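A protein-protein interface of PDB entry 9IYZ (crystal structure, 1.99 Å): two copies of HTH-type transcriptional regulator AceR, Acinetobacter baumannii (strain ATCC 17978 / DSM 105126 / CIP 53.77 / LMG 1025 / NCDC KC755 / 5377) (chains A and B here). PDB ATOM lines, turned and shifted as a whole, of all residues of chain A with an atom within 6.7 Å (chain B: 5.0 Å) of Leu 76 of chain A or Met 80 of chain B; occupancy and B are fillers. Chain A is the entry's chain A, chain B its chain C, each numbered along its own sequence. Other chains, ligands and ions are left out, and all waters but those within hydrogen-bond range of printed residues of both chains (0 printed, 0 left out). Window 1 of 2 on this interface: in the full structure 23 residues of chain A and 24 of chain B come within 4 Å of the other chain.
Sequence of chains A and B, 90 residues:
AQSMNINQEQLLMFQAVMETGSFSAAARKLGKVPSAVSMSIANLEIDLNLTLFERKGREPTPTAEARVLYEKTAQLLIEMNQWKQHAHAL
Among the printed residues, pairs that only touch across the chains: Leu 11 of chain A with Trp 83 of chain B (3.6 Å), Lys 72 of chain A with Trp 83 of chain B (3.9 Å), Gln 75 of chain A with Glu 79 of chain B (3.5 Å), Leu 76 of chain A with Leu 76 of chain B (3.7 Å), Leu 76 of chain A with Met 80 of chain B (3.8 Å), Leu 76 of chain A with Trp 83 of chain B (3.6 Å), Glu 79 of chain A with Leu 76 of chain B (3.9 Å), Glu 79 of chain A with Glu 79 of chain B (3.3 Å) and Met 80 of chain A with Leu 76 of chain B (3.96 Å).
Hydrophobic or aromatic side chains of chain B within 4 Å of the printed part of chain A: Leu 76, Met 80 and Trp 83.
Of the 12 printed residues of chain A, 7 touch a printed residue of chain B.
Hydrophobic or aromatic side chains of chain A that line the printed part of chain B: Leu 11, Leu 76 and Met 80.
Among the printed residues, no Asp or Glu carboxylate lies within 4 Å of a Lys or Arg side-chain nitrogen of the other chain.
Leu 76 of chain A touches three residues of chain B.
Met 80 of chain B touches just one residue of chain A: Leu 76.
Of the printed residues of chain A, Trp 83 of chain B touches Leu 11 (3.6 Å), Lys 72 (3.9 Å), Thr 73 (2.9 Å) and Leu 76 (3.6 Å).
Printed residues of chain B within 4 Å of Lys 72 of chain A: Trp 83 (3.9 Å).
Of the printed residues of chain B, Thr 73 of chain A touches Trp 83.
Printed residues of chain A within 4 Å of Glu 79 of chain B: Gln 75 and Glu 79.
Gln 82 of chain B touches none of the printed residues of chain A.
Leu 12 of chain B touches none of the printed residues of chain A.
The nearest residue of chain B that does not touch Leu 76 of chain A is Glu 79 of chain B (4.1 Å).
The nearest residue of chain A that does not touch Met 80 of chain B is Met 80 of chain A (4.8 Å).
Leu 76 of chain A touches its own counterpart, Leu 76 of chain B.
Leu 76 of chain A touches Met 80 of chain B, and with the chains exchanged Met 80 of chain A touches Leu 76 of chain B.
Glu 79 of chain A touches Leu 76 of chain B, but with the chains exchanged Leu 76 of chain A does not touch Glu 79 of chain B (4.1 Å).
Glu 79 of chain A touches its own counterpart, Glu 79 of chain B.
Of the 10 pairs that touch across the chains among the printed residues, 4 have their exchanged pair printed and touching as well.
The side-chain hydroxyl (OG1) of Thr 73 of chain A lies within hydrogen-bond range of the indole nitrogen (NE1) of Trp 83 of chain B, 2.9 Å away.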
ATOM      1  N   LEU A  11      -1.547   6.926   8.557  1.00  0.00           N
ATOM      2  CA  LEU A  11      -2.797   6.998   7.808  1.00  0.00           C
ATOM      3  C   LEU A  11      -3.857   7.778   8.579  1.00  0.00           C
ATOM      4  O   LEU A  11      -4.648   8.520   7.985  1.00  0.00           O
ATOM      5  CB  LEU A  11      -3.278   5.586   7.482  1.00  0.00           C
ATOM      6  CG  LEU A  11      -2.357   4.791   6.543  1.00  0.00           C
ATOM      7  CD1 LEU A  11      -3.071   3.555   6.013  1.00  0.00           C
ATOM      8  CD2 LEU A  11      -1.868   5.648   5.389  1.00  0.00           C
ATOM      9  N   GLU A  71      -9.588   8.322  -0.295  1.00  0.00           N
ATOM     10  CA  GLU A  71     -10.751   7.481  -0.516  1.00  0.00           C
ATOM     11  C   GLU A  71     -10.436   6.036  -0.160  1.00  0.00           C
ATOM     12  O   GLU A  71     -11.154   5.407   0.628  1.00  0.00           O
ATOM     13  CB  GLU A  71     -11.195   7.600  -1.971  1.00  0.00           C
ATOM     14  CG  GLU A  71     -12.494   6.909  -2.277  1.00  0.00           C
ATOM     15  CD  GLU A  71     -13.113   7.421  -3.549  1.00  0.00           C
ATOM     16  OE1 GLU A  71     -13.051   8.646  -3.783  1.00  0.00           O
ATOM     17  OE2 GLU A  71     -13.659   6.601  -4.319  1.00  0.00           O
ATOM     18  N   LYS A  72      -9.338   5.506  -0.705  1.00  0.00           N
ATOM     19  CA  LYS A  72      -8.989   4.111  -0.456  1.00  0.00           C
ATOM     20  C   LYS A  72      -8.496   3.893   0.966  1.00  0.00           C
ATOM     21  O   LYS A  72      -8.635   2.793   1.508  1.00  0.00           O
ATOM     22  CB  LYS A  72      -7.956   3.659  -1.479  1.00  0.00           C
ATOM     23  CG  LYS A  72      -8.296   4.163  -2.875  1.00  0.00           C
ATOM     24  CD  LYS A  72      -9.259   3.209  -3.547  1.00  0.00           C
ATOM     25  CE  LYS A  72      -9.845   3.785  -4.820  1.00  0.00           C
ATOM     26  NZ  LYS A  72     -11.177   3.165  -5.111  1.00  0.00           N
ATOM     27  N   THR A  73      -7.937   4.922   1.595  1.00  0.00           N
ATOM     28  CA  THR A  73      -7.509   4.773   2.978  1.00  0.00           C
ATOM     29  C   THR A  73      -8.701   4.553   3.900  1.00  0.00           C
ATOM     30  O   THR A  73      -8.567   3.916   4.952  1.00  0.00           O
ATOM     31  CB  THR A  73      -6.701   6.001   3.387  1.00  0.00           C
ATOM     32  OG1 THR A  73      -5.545   6.091   2.543  1.00  0.00           O
ATOM     33  CG2 THR A  73      -6.256   5.911   4.838  1.00  0.00           C
ATOM     34  N   ALA A  74      -9.881   5.040   3.504  1.00  0.00           N
ATOM     35  CA  ALA A  74     -11.069   4.906   4.342  1.00  0.00           C
ATOM     36  C   ALA A  74     -11.477   3.447   4.507  1.00  0.00           C
ATOM     37  O   ALA A  74     -11.833   3.019   5.609  1.00  0.00           O
ATOM     38  CB  ALA A  74     -12.216   5.726   3.748  1.00  0.00           C
ATOM     39  N   GLN A  75     -11.429   2.670   3.426  1.00  0.00           N
ATOM     40  CA  GLN A  75     -11.760   1.253   3.514  1.00  0.00           C
ATOM     41  C   GLN A  75     -10.732   0.485   4.336  1.00  0.00           C
ATOM     42  O   GLN A  75     -11.072  -0.470   5.046  1.00  0.00           O
ATOM     43  CB  GLN A  75     -11.853   0.658   2.112  1.00  0.00           C
ATOM     44  CG  GLN A  75     -12.295  -0.799   2.069  1.00  0.00           C
ATOM     45  CD  GLN A  75     -13.454  -1.103   3.019  1.00  0.00           C
ATOM     46  OE1 GLN A  75     -13.278  -1.761   4.053  1.00  0.00           O
ATOM     47  NE2 GLN A  75     -14.647  -0.625   2.667  1.00  0.00           N
ATOM     48  N   LEU A  76      -9.462   0.853   4.212  1.00  0.00           N
ATOM     49  CA  LEU A  76      -8.435   0.172   4.979  1.00  0.00           C
ATOM     50  C   LEU A  76      -8.530   0.552   6.447  1.00  0.00           C
ATOM     51  O   LEU A  76      -8.228  -0.267   7.324  1.00  0.00           O
ATOM     52  CB  LEU A  76      -7.055   0.512   4.410  1.00  0.00           C
ATOM     53  CG  LEU A  76      -5.830   0.121   5.232  1.00  0.00           C
ATOM     54  CD1 LEU A  76      -5.873  -1.375   5.503  1.00  0.00           C
ATOM     55  CD2 LEU A  76      -4.563   0.483   4.483  1.00  0.00           C
ATOM     56  N   LEU A  77      -8.958   1.783   6.733  1.00  0.00           N
ATOM     57  CA  LEU A  77      -9.101   2.208   8.123  1.00  0.00           C
ATOM     58  C   LEU A  77     -10.221   1.448   8.818  1.00  0.00           C
ATOM     59  O   LEU A  77     -10.087   1.085   9.990  1.00  0.00           O
ATOM     60  CB  LEU A  77      -9.330   3.715   8.191  1.00  0.00           C
ATOM     61  CG  LEU A  77      -8.026   4.510   8.088  1.00  0.00           C
ATOM     62  CD1 LEU A  77      -8.310   5.969   7.804  1.00  0.00           C
ATOM     63  CD2 LEU A  77      -7.227   4.347   9.368  1.00  0.00           C
ATOM     64  N   ILE A  78     -11.313   1.161   8.105  1.00  0.00           N
ATOM     65  CA  ILE A  78     -12.344   0.263   8.631  1.00  0.00           C
ATOM     66  C   ILE A  78     -11.724  -1.050   9.094  1.00  0.00           C
ATOM     67  O   ILE A  78     -11.924  -1.486  10.233  1.00  0.00           O
ATOM     68  CB  ILE A  78     -13.425  -0.005   7.572  1.00  0.00           C
ATOM     69  CG1 ILE A  78     -14.280   1.234   7.309  1.00  0.00           C
ATOM     70  CG2 ILE A  78     -14.316  -1.147   8.016  1.00  0.00           C
ATOM     71  CD1 ILE A  78     -15.239   1.006   6.179  1.00  0.00           C
ATOM     72  N   GLU A  79     -10.978  -1.707   8.197  1.00  0.00           N
ATOM     73  CA  GLU A  79     -10.399  -3.014   8.498  1.00  0.00           C
ATOM     74  C   GLU A  79      -9.348  -2.939   9.595  1.00  0.00           C
ATOM     75  O   GLU A  79      -9.222  -3.876  10.390  1.00  0.00           O
ATOM     76  CB  GLU A  79      -9.793  -3.629   7.237  1.00  0.00           C
ATOM     77  CG  GLU A  79     -10.811  -4.078   6.218  1.00  0.00           C
ATOM     78  CD  GLU A  79     -11.780  -5.094   6.768  1.00  0.00           C
ATOM     79  OE1 GLU A  79     -11.324  -6.134   7.304  1.00  0.00           O
ATOM     80  OE2 GLU A  79     -13.001  -4.847   6.664  1.00  0.00           O
ATOM     81  N   MET A  80      -8.552  -1.861   9.638  1.00  0.00           N
ATOM     82  CA  MET A  80      -7.545  -1.747  10.697  1.00  0.00           C
ATOM     83  C   MET A  80      -8.197  -1.697  12.074  1.00  0.00           C
ATOM     84  O   MET A  80      -7.742  -2.361  13.015  1.00  0.00           O
ATOM     85  CB  MET A  80      -6.669  -0.508  10.496  1.00  0.00           C
ATOM     86  CG  MET A  80      -5.419  -0.751   9.672  1.00  0.00           C
ATOM     87  SD  MET A  80      -4.574   0.781   9.237  1.00  0.00           S
ATOM     88  CE  MET A  80      -3.214   0.128   8.252  1.00  0.00           C
ATOM     89  N   ASN A  81      -9.271  -0.922  12.211  1.00  0.00           N
ATOM     90  CA  ASN A  81      -9.974  -0.849  13.490  1.00  0.00           C
ATOM     91  C   ASN A  81     -10.662  -2.168  13.820  1.00  0.00           C
ATOM     92  O   ASN A  81     -10.677  -2.593  14.983  1.00  0.00           O
ATOM     93  CB  ASN A  81     -10.998   0.285  13.458  1.00  0.00           C
ATOM     94  CG  ASN A  81     -10.563   1.481  14.266  1.00  0.00           C
ATOM     95  OD1 ASN A  81     -10.414   1.400  15.487  1.00  0.00           O
ATOM     96  ND2 ASN A  81     -10.368   2.611  13.591  1.00  0.00           N
ATOM     97  N   GLN B   8       2.526  -2.444   9.266  1.00  0.00           N
ATOM     98  CA  GLN B   8       2.239  -3.521   8.327  1.00  0.00           C
ATOM     99  C   GLN B   8       3.344  -4.556   8.286  1.00  0.00           C
ATOM    100  O   GLN B   8       3.060  -5.754   8.178  1.00  0.00           O
ATOM    101  CB  GLN B   8       2.010  -2.966   6.926  1.00  0.00           C
ATOM    102  CG  GLN B   8       1.223  -1.668   6.900  1.00  0.00           C
ATOM    103  CD  GLN B   8       1.080  -1.099   5.494  1.00  0.00           C
ATOM    104  OE1 GLN B   8       2.081  -0.795   4.838  1.00  0.00           O
ATOM    105  NE2 GLN B   8      -0.166  -0.958   5.024  1.00  0.00           N
ATOM    106  N   LEU B  11       2.935  -7.305  10.692  1.00  0.00           N
ATOM    107  CA  LEU B  11       1.885  -8.265  10.385  1.00  0.00           C
ATOM    108  C   LEU B  11       2.324  -9.228   9.284  1.00  0.00           C
ATOM    109  O   LEU B  11       2.036 -10.427   9.356  1.00  0.00           O
ATOM    110  CB  LEU B  11       0.607  -7.501  10.020  1.00  0.00           C
ATOM    111  CG  LEU B  11       0.002  -6.710  11.192  1.00  0.00           C
ATOM    112  CD1 LEU B  11      -1.468  -6.336  10.963  1.00  0.00           C
ATOM    113  CD2 LEU B  11       0.126  -7.483  12.506  1.00  0.00           C
ATOM    114  N   LEU B  12       3.045  -8.727   8.270  1.00  0.00           N
ATOM    115  CA  LEU B  12       3.550  -9.597   7.210  1.00  0.00           C
ATOM    116  C   LEU B  12       4.533 -10.605   7.768  1.00  0.00           C
ATOM    117  O   LEU B  12       4.527 -11.781   7.386  1.00  0.00           O
ATOM    118  CB  LEU B  12       4.235  -8.779   6.116  1.00  0.00           C
ATOM    119  CG  LEU B  12       3.431  -8.460   4.853  1.00  0.00           C
ATOM    120  CD1 LEU B  12       3.302  -9.697   3.980  1.00  0.00           C
ATOM    121  CD2 LEU B  12       2.086  -7.929   5.225  1.00  0.00           C
ATOM    122  N   LEU B  76      -7.393  -8.464   7.142  1.00  0.00           N
ATOM    123  CA  LEU B  76      -6.793  -7.143   7.011  1.00  0.00           C
ATOM    124  C   LEU B  76      -5.757  -7.123   5.898  1.00  0.00           C
ATOM    125  O   LEU B  76      -5.628  -6.123   5.190  1.00  0.00           O
ATOM    126  CB  LEU B  76      -6.163  -6.716   8.339  1.00  0.00           C
ATOM    127  CG  LEU B  76      -5.244  -5.491   8.368  1.00  0.00           C
ATOM    128  CD1 LEU B  76      -5.944  -4.226   7.818  1.00  0.00           C
ATOM    129  CD2 LEU B  76      -4.706  -5.237   9.765  1.00  0.00           C
ATOM    130  N   LEU B  77      -5.039  -8.229   5.695  1.00  0.00           N
ATOM    131  CA  LEU B  77      -3.993  -8.228   4.671  1.00  0.00           C
ATOM    132  C   LEU B  77      -4.574  -8.095   3.268  1.00  0.00           C
ATOM    133  O   LEU B  77      -3.921  -7.528   2.386  1.00  0.00           O
ATOM    134  CB  LEU B  77      -3.148  -9.501   4.746  1.00  0.00           C
ATOM    135  CG  LEU B  77      -2.161  -9.670   5.895  1.00  0.00           C
ATOM    136  CD1 LEU B  77      -1.170 -10.733   5.518  1.00  0.00           C
ATOM    137  CD2 LEU B  77      -1.465  -8.403   6.240  1.00  0.00           C
ATOM    138  N   ILE B  78      -5.776  -8.631   3.033  1.00  0.00           N
ATOM    139  CA  ILE B  78      -6.445  -8.416   1.748  1.00  0.00           C
ATOM    140  C   ILE B  78      -6.549  -6.923   1.458  1.00  0.00           C
ATOM    141  O   ILE B  78      -6.225  -6.455   0.359  1.00  0.00           O
ATOM    142  CB  ILE B  78      -7.838  -9.073   1.743  1.00  0.00           C
ATOM    143  CG1 ILE B  78      -7.747 -10.603   1.839  1.00  0.00           C
ATOM    144  CG2 ILE B  78      -8.642  -8.622   0.522  1.00  0.00           C
ATOM    145  CD1 ILE B  78      -9.084 -11.254   2.082  1.00  0.00           C
ATOM    146  N   GLU B  79      -7.000  -6.151   2.451  1.00  0.00           N
ATOM    147  CA  GLU B  79      -7.165  -4.712   2.249  1.00  0.00           C
ATOM    148  C   GLU B  79      -5.833  -3.983   2.197  1.00  0.00           C
ATOM    149  O   GLU B  79      -5.688  -3.017   1.440  1.00  0.00           O
ATOM    150  CB  GLU B  79      -8.054  -4.124   3.334  1.00  0.00           C
ATOM    151  CG  GLU B  79      -9.456  -4.634   3.232  1.00  0.00           C
ATOM    152  CD  GLU B  79     -10.163  -4.115   1.991  1.00  0.00           C
ATOM    153  OE1 GLU B  79     -11.165  -4.738   1.578  1.00  0.00           O
ATOM    154  OE2 GLU B  79      -9.731  -3.070   1.451  1.00  0.00           O
ATOM    155  N   MET B  80      -4.846  -4.405   2.991  1.00  0.00           N
ATOM    156  CA  MET B  80      -3.588  -3.666   2.935  1.00  0.00           C
ATOM    157  C   MET B  80      -2.987  -3.782   1.548  1.00  0.00           C
ATOM    158  O   MET B  80      -2.424  -2.814   1.031  1.00  0.00           O
ATOM    159  CB  MET B  80      -2.571  -4.168   3.957  1.00  0.00           C
ATOM    160  CG  MET B  80      -2.805  -3.682   5.380  1.00  0.00           C
ATOM    161  SD  MET B  80      -1.631  -4.417   6.536  1.00  0.00           S
ATOM    162  CE  MET B  80      -0.591  -5.345   5.415  1.00  0.00           C
ATOM    163  N   ASN B  81      -3.162  -4.944   0.919  1.00  0.00           N
ATOM    164  CA  ASN B  81      -2.626  -5.185  -0.415  1.00  0.00           C
ATOM    165  C   ASN B  81      -3.295  -4.297  -1.449  1.00  0.00           C
ATOM    166  O   ASN B  81      -2.623  -3.733  -2.319  1.00  0.00           O
ATOM    167  CB  ASN B  81      -2.816  -6.652  -0.777  1.00  0.00           C
ATOM    168  CG  ASN B  81      -1.681  -7.500  -0.292  1.00  0.00           C
ATOM    169  OD1 ASN B  81      -0.611  -6.984   0.025  1.00  0.00           O
ATOM    170  ND2 ASN B  81      -1.912  -8.803  -0.188  1.00  0.00           N
ATOM    171  N   GLN B  82      -4.625  -4.186  -1.384  1.00  0.00           N
ATOM    172  CA  GLN B  82      -5.336  -3.319  -2.318  1.00  0.00           C
ATOM    173  C   GLN B  82      -4.893  -1.877  -2.184  1.00  0.00           C
ATOM    174  O   GLN B  82      -4.753  -1.168  -3.186  1.00  0.00           O
ATOM    175  CB  GLN B  82      -6.845  -3.429  -2.114  1.00  0.00           C
ATOM    176  CG  GLN B  82      -7.321  -4.839  -2.198  1.00  0.00           C
ATOM    177  CD  GLN B  82      -7.329  -5.276  -3.633  1.00  0.00           C
ATOM    178  OE1 GLN B  82      -6.685  -6.260  -3.998  1.00  0.00           O
ATOM    179  NE2 GLN B  82      -8.031  -4.518  -4.475  1.00  0.00           N
ATOM    180  N   TRP B  83      -4.691  -1.419  -0.953  1.00  0.00           N
ATOM    181  CA  TRP B  83      -4.275  -0.040  -0.741  1.00  0.00           C
ATOM    182  C   TRP B  83      -2.901   0.201  -1.350  1.00  0.00           C
ATOM    183  O   TRP B  83      -2.682   1.210  -2.030  1.00  0.00           O
ATOM    184  CB  TRP B  83      -4.288   0.269   0.759  1.00  0.00           C
ATOM    185  CG  TRP B  83      -3.908   1.665   1.108  1.00  0.00           C
ATOM    186  CD1 TRP B  83      -4.726   2.761   1.137  1.00  0.00           C
ATOM    187  CD2 TRP B  83      -2.611   2.120   1.493  1.00  0.00           C
ATOM    188  NE1 TRP B  83      -4.005   3.879   1.506  1.00  0.00           N
ATOM    189  CE2 TRP B  83      -2.705   3.507   1.734  1.00  0.00           C
ATOM    190  CE3 TRP B  83      -1.375   1.489   1.648  1.00  0.00           C
ATOM    191  CZ2 TRP B  83      -1.610   4.272   2.124  1.00  0.00           C
ATOM    192  CZ3 TRP B  83      -0.288   2.249   2.034  1.00  0.00           C
ATOM    193  CH2 TRP B  83      -0.415   3.628   2.269  1.00  0.00           C
ATOM    194  N   LYS B  84      -1.976  -0.744  -1.149  1.00  0.00           N
ATOM    195  CA  LYS B  84      -0.618  -0.612  -1.670  1.00  0.00           C
ATOM    196  C   LYS B  84      -0.605  -0.643  -3.191  1.00  0.00           C
ATOM    197  O   LYS B  84       0.190   0.060  -3.823  1.00  0.00           O
ATOM    198  CB  LYS B  84       0.264  -1.731  -1.106  1.00  0.00           C
ATOM    199  CG  LYS B  84       0.173  -1.843   0.394  1.00  0.00           C
ATOM    200  CD  LYS B  84       1.383  -2.440   1.060  1.00  0.00           C
ATOM    201  CE  LYS B  84       0.960  -3.644   1.920  1.00  0.00           C
ATOM    202  NZ  LYS B  84       1.903  -3.996   3.029  1.00  0.00           N
